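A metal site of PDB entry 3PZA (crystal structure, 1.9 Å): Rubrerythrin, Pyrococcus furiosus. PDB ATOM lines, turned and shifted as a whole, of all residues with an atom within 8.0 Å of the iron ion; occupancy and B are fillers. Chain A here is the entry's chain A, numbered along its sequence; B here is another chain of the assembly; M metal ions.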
ATOM      1  N   TYR A 108     -28.235 -14.565 -15.207  1.00  0.00           N
ATOM      2  CA  TYR A 108     -26.942 -14.765 -15.864  1.00  0.00           C
ATOM      3  C   TYR A 108     -25.944 -15.313 -14.885  1.00  0.00           C
ATOM      4  O   TYR A 108     -25.192 -16.223 -15.181  1.00  0.00           O
ATOM      5  CB  TYR A 108     -26.413 -13.429 -16.355  1.00  0.00           C
ATOM      6  CG  TYR A 108     -27.081 -12.881 -17.598  1.00  0.00           C
ATOM      7  CD1 TYR A 108     -28.045 -13.650 -18.315  1.00  0.00           C
ATOM      8  CD2 TYR A 108     -26.662 -11.631 -18.138  1.00  0.00           C
ATOM      9  CE1 TYR A 108     -28.620 -13.163 -19.531  1.00  0.00           C
ATOM     10  CE2 TYR A 108     -27.253 -11.144 -19.369  1.00  0.00           C
ATOM     11  CZ  TYR A 108     -28.177 -11.940 -20.044  1.00  0.00           C
ATOM     12  OH  TYR A 108     -28.742 -11.479 -21.219  1.00  0.00           O
ATOM     13  N   ILE A 140     -14.989 -17.603 -22.078  1.00  0.00           N
ATOM     14  CA  ILE A 140     -15.980 -16.919 -21.195  1.00  0.00           C
ATOM     15  C   ILE A 140     -16.868 -16.025 -22.003  1.00  0.00           C
ATOM     16  O   ILE A 140     -16.351 -15.162 -22.756  1.00  0.00           O
ATOM     17  CB  ILE A 140     -15.254 -16.070 -20.027  1.00  0.00           C
ATOM     18  CG1 ILE A 140     -14.215 -16.861 -19.273  1.00  0.00           C
ATOM     19  CG2 ILE A 140     -16.301 -15.511 -19.077  1.00  0.00           C
ATOM     20  CD1 ILE A 140     -14.738 -18.026 -18.346  1.00  0.00           C
ATOM     21  N   CYS A 141     -18.211 -16.107 -21.802  1.00  0.00           N
ATOM     22  CA  CYS A 141     -19.064 -15.177 -22.463  1.00  0.00           C
ATOM     23  C   CYS A 141     -18.937 -13.762 -21.801  1.00  0.00           C
ATOM     24  O   CYS A 141     -19.182 -13.635 -20.621  1.00  0.00           O
ATOM     25  CB  CYS A 141     -20.513 -15.702 -22.479  1.00  0.00           C
ATOM     26  SG  CYS A 141     -21.710 -14.542 -23.221  1.00  0.00           S
ATOM     27  N   PRO A 142     -18.643 -12.723 -22.608  1.00  0.00           N
ATOM     28  CA  PRO A 142     -18.503 -11.374 -22.042  1.00  0.00           C
ATOM     29  C   PRO A 142     -19.850 -10.705 -21.745  1.00  0.00           C
ATOM     30  O   PRO A 142     -19.857  -9.626 -21.121  1.00  0.00           O
ATOM     31  CB  PRO A 142     -17.700 -10.629 -23.122  1.00  0.00           C
ATOM     32  CG  PRO A 142     -18.307 -11.179 -24.449  1.00  0.00           C
ATOM     33  CD  PRO A 142     -18.409 -12.721 -24.080  1.00  0.00           C
ATOM     34  N   ILE A 143     -20.998 -11.320 -22.090  1.00  0.00           N
ATOM     35  CA  ILE A 143     -22.298 -10.749 -21.738  1.00  0.00           C
ATOM     36  C   ILE A 143     -22.841 -11.321 -20.393  1.00  0.00           C
ATOM     37  O   ILE A 143     -23.304 -10.578 -19.522  1.00  0.00           O
ATOM     38  CB  ILE A 143     -23.334 -11.003 -22.880  1.00  0.00           C
ATOM     39  CG1 ILE A 143     -22.809 -10.449 -24.257  1.00  0.00           C
ATOM     40  CG2 ILE A 143     -24.711 -10.523 -22.528  1.00  0.00           C
ATOM     41  CD1 ILE A 143     -22.347  -9.078 -24.235  1.00  0.00           C
ATOM     42  N   CYS A 144     -22.698 -12.618 -20.164  1.00  0.00           N
ATOM     43  CA  CYS A 144     -23.325 -13.237 -18.987  1.00  0.00           C
ATOM     44  C   CYS A 144     -22.354 -14.091 -18.197  1.00  0.00           C
ATOM     45  O   CYS A 144     -22.723 -14.585 -17.137  1.00  0.00           O
ATOM     46  CB  CYS A 144     -24.550 -14.126 -19.460  1.00  0.00           C
ATOM     47  SG  CYS A 144     -23.941 -15.665 -20.365  1.00  0.00           S
ATOM     48  N   GLY A 145     -21.106 -14.246 -18.646  1.00  0.00           N
ATOM     49  CA  GLY A 145     -20.141 -15.028 -17.868  1.00  0.00           C
ATOM     50  C   GLY A 145     -20.265 -16.541 -17.980  1.00  0.00           C
ATOM     51  O   GLY A 145     -19.533 -17.353 -17.292  1.00  0.00           O
ATOM     52  N   TYR A 146     -21.133 -16.972 -18.910  1.00  0.00           N
ATOM     53  CA  TYR A 146     -21.151 -18.417 -19.246  1.00  0.00           C
ATOM     54  C   TYR A 146     -19.705 -18.931 -19.483  1.00  0.00           C
ATOM     55  O   TYR A 146     -18.947 -18.229 -20.179  1.00  0.00           O
ATOM     56  CB  TYR A 146     -21.969 -18.634 -20.526  1.00  0.00           C
ATOM     57  CG  TYR A 146     -21.804 -20.056 -21.036  1.00  0.00           C
ATOM     58  CD1 TYR A 146     -21.031 -20.248 -22.204  1.00  0.00           C
ATOM     59  CD2 TYR A 146     -22.411 -21.190 -20.367  1.00  0.00           C
ATOM     60  CE1 TYR A 146     -20.863 -21.537 -22.748  1.00  0.00           C
ATOM     61  CE2 TYR A 146     -22.230 -22.520 -20.910  1.00  0.00           C
ATOM     62  CZ  TYR A 146     -21.437 -22.612 -22.123  1.00  0.00           C
ATOM     63  OH  TYR A 146     -21.177 -23.848 -22.720  1.00  0.00           O
ATOM     64  N   THR A 147     -19.340 -20.124 -18.995  1.00  0.00           N
ATOM     65  CA  THR A 147     -17.917 -20.585 -18.989  1.00  0.00           C
ATOM     66  C   THR A 147     -17.890 -21.965 -19.627  1.00  0.00           C
ATOM     67  O   THR A 147     -18.762 -22.809 -19.291  1.00  0.00           O
ATOM     68  CB  THR A 147     -17.498 -20.712 -17.530  1.00  0.00           C
ATOM     69  OG1 THR A 147     -17.564 -19.386 -16.942  1.00  0.00           O
ATOM     70  CG2 THR A 147     -16.073 -21.269 -17.344  1.00  0.00           C
ATOM     71  N   TYR A 155     -23.260 -20.937 -29.929  1.00  0.00           N
ATOM     72  CA  TYR A 155     -23.928 -19.765 -29.312  1.00  0.00           C
ATOM     73  C   TYR A 155     -24.012 -19.999 -27.784  1.00  0.00           C
ATOM     74  O   TYR A 155     -24.200 -21.118 -27.321  1.00  0.00           O
ATOM     75  CB  TYR A 155     -25.399 -19.597 -29.800  1.00  0.00           C
ATOM     76  CG  TYR A 155     -25.363 -19.292 -31.281  1.00  0.00           C
ATOM     77  CD1 TYR A 155     -25.145 -17.990 -31.729  1.00  0.00           C
ATOM     78  CD2 TYR A 155     -25.364 -20.332 -32.229  1.00  0.00           C
ATOM     79  CE1 TYR A 155     -25.002 -17.742 -33.070  1.00  0.00           C
ATOM     80  CE2 TYR A 155     -25.273 -20.044 -33.626  1.00  0.00           C
ATOM     81  CZ  TYR A 155     -25.087 -18.770 -34.004  1.00  0.00           C
ATOM     82  OH  TYR A 155     -25.014 -18.467 -35.377  1.00  0.00           O
ATOM     83  N   CYS A 156     -23.845 -18.931 -27.013  1.00  0.00           N
ATOM     84  CA  CYS A 156     -23.973 -18.996 -25.528  1.00  0.00           C
ATOM     85  C   CYS A 156     -25.355 -19.551 -25.189  1.00  0.00           C
ATOM     86  O   CYS A 156     -26.349 -18.995 -25.694  1.00  0.00           O
ATOM     87  CB  CYS A 156     -23.959 -17.522 -24.999  1.00  0.00           C
ATOM     88  SG  CYS A 156     -24.076 -17.634 -23.186  1.00  0.00           S
ATOM     89  N   PRO A 157     -25.473 -20.610 -24.374  1.00  0.00           N
ATOM     90  CA  PRO A 157     -26.867 -21.135 -24.092  1.00  0.00           C
ATOM     91  C   PRO A 157     -27.724 -20.223 -23.189  1.00  0.00           C
ATOM     92  O   PRO A 157     -28.993 -20.353 -23.110  1.00  0.00           O
ATOM     93  CB  PRO A 157     -26.624 -22.441 -23.363  1.00  0.00           C
ATOM     94  CG  PRO A 157     -25.214 -22.260 -22.707  1.00  0.00           C
ATOM     95  CD  PRO A 157     -24.435 -21.353 -23.668  1.00  0.00           C
ATOM     96  N   VAL A 158     -27.068 -19.221 -22.574  1.00  0.00           N
ATOM     97  CA  VAL A 158     -27.835 -18.355 -21.635  1.00  0.00           C
ATOM     98  C   VAL A 158     -28.295 -17.085 -22.338  1.00  0.00           C
ATOM     99  O   VAL A 158     -29.493 -16.720 -22.252  1.00  0.00           O
ATOM    100  CB  VAL A 158     -26.918 -17.983 -20.408  1.00  0.00           C
ATOM    101  CG1 VAL A 158     -27.655 -16.939 -19.467  1.00  0.00           C
ATOM    102  CG2 VAL A 158     -26.512 -19.214 -19.678  1.00  0.00           C
ATOM    103  N   CYS A 159     -27.425 -16.393 -23.063  1.00  0.00           N
ATOM    104  CA  CYS A 159     -27.825 -15.136 -23.704  1.00  0.00           C
ATOM    105  C   CYS A 159     -27.852 -15.184 -25.238  1.00  0.00           C
ATOM    106  O   CYS A 159     -28.155 -14.164 -25.877  1.00  0.00           O
ATOM    107  CB  CYS A 159     -26.899 -13.968 -23.312  1.00  0.00           C
ATOM    108  SG  CYS A 159     -25.167 -14.057 -23.862  1.00  0.00           S
ATOM    109  N   GLY A 160     -27.348 -16.285 -25.798  1.00  0.00           N
ATOM    110  CA  GLY A 160     -27.325 -16.390 -27.262  1.00  0.00           C
ATOM    111  C   GLY A 160     -26.158 -15.738 -28.011  1.00  0.00           C
ATOM    112  O   GLY A 160     -26.121 -15.769 -29.267  1.00  0.00           O
ATOM    113  N   ALA A 161     -25.178 -15.180 -27.304  1.00  0.00           N
ATOM    114  CA  ALA A 161     -24.003 -14.506 -27.947  1.00  0.00           C
ATOM    115  C   ALA A 161     -23.217 -15.521 -28.799  1.00  0.00           C
ATOM    116  O   ALA A 161     -23.009 -16.666 -28.375  1.00  0.00           O
ATOM    117  CB  ALA A 161     -23.041 -13.994 -26.914  1.00  0.00           C
ATOM    118  N   PRO A 162     -22.723 -15.076 -29.971  1.00  0.00           N
ATOM    119  CA  PRO A 162     -21.963 -16.093 -30.778  1.00  0.00           C
ATOM    120  C   PRO A 162     -20.585 -16.373 -30.161  1.00  0.00           C
ATOM    121  O   PRO A 162     -20.000 -15.501 -29.508  1.00  0.00           O
ATOM    122  CB  PRO A 162     -21.748 -15.388 -32.151  1.00  0.00           C
ATOM    123  CG  PRO A 162     -22.120 -13.973 -31.951  1.00  0.00           C
ATOM    124  CD  PRO A 162     -23.014 -13.836 -30.714  1.00  0.00           C
ATOM    125  N   PHE A 166     -16.648 -14.812 -27.467  1.00  0.00           N
ATOM    126  CA  PHE A 166     -16.159 -15.299 -26.211  1.00  0.00           C
ATOM    127  C   PHE A 166     -14.708 -14.920 -25.997  1.00  0.00           C
ATOM    128  O   PHE A 166     -13.893 -14.977 -26.935  1.00  0.00           O
ATOM    129  CB  PHE A 166     -16.247 -16.847 -26.012  1.00  0.00           C
ATOM    130  CG  PHE A 166     -17.633 -17.408 -26.117  1.00  0.00           C
ATOM    131  CD1 PHE A 166     -18.747 -16.585 -26.010  1.00  0.00           C
ATOM    132  CD2 PHE A 166     -17.780 -18.839 -26.343  1.00  0.00           C
ATOM    133  CE1 PHE A 166     -20.071 -17.153 -26.094  1.00  0.00           C
ATOM    134  CE2 PHE A 166     -19.047 -19.422 -26.426  1.00  0.00           C
ATOM    135  CZ  PHE A 166     -20.213 -18.596 -26.300  1.00  0.00           C
ATOM    136  N   VAL B  53     -17.610 -10.049 -15.345  1.00  0.00           N
ATOM    137  CA  VAL B  53     -18.795  -9.890 -16.141  1.00  0.00           C
ATOM    138  C   VAL B  53     -20.028  -9.818 -15.229  1.00  0.00           C
ATOM    139  O   VAL B  53     -20.892  -8.875 -15.390  1.00  0.00           O
ATOM    140  CB  VAL B  53     -18.918 -11.058 -17.145  1.00  0.00           C
ATOM    141  CG1 VAL B  53     -20.280 -10.896 -17.936  1.00  0.00           C
ATOM    142  CG2 VAL B  53     -17.816 -10.976 -18.159  1.00  0.00           C
HETATM  143 FE    FE M   1     -23.759 -15.442 -22.633  1.00  0.00          FE
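The side-chain sulfur (SG) of Cys 141 sits close to the backbone NH (N) of Ile 143 (3.5 Å).
N of Tyr 146 lies close to SG of Cys 144.
The backbone NH (N) of Ala 161 sits close to the side-chain sulfur (SG) of Cys 159 (3.6 Å).
SG of Cys 156 lies close to N of Val 158 (3.4 Å).
O of Tyr 146 sits at hydrogen-bond distance from N of Cys 141, 2.8 Å away.
The backbone carbonyl oxygen (O) of Ala 161 lies within hydrogen-bond range of the backbone NH (N) of Cys 156 (2.8 Å).
The nearest printed residue that does not touch the iron ion is Tyr 146 (4.2 Å).
SG of Cys 156 binds the iron ion.
The iron ion is bound by SG of Cys 144 (2.3 Å).
SG of Cys 141 is bound to the iron ion, 2.3 Å away.
SG of Cys 159 binds the iron ion (2.3 Å).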
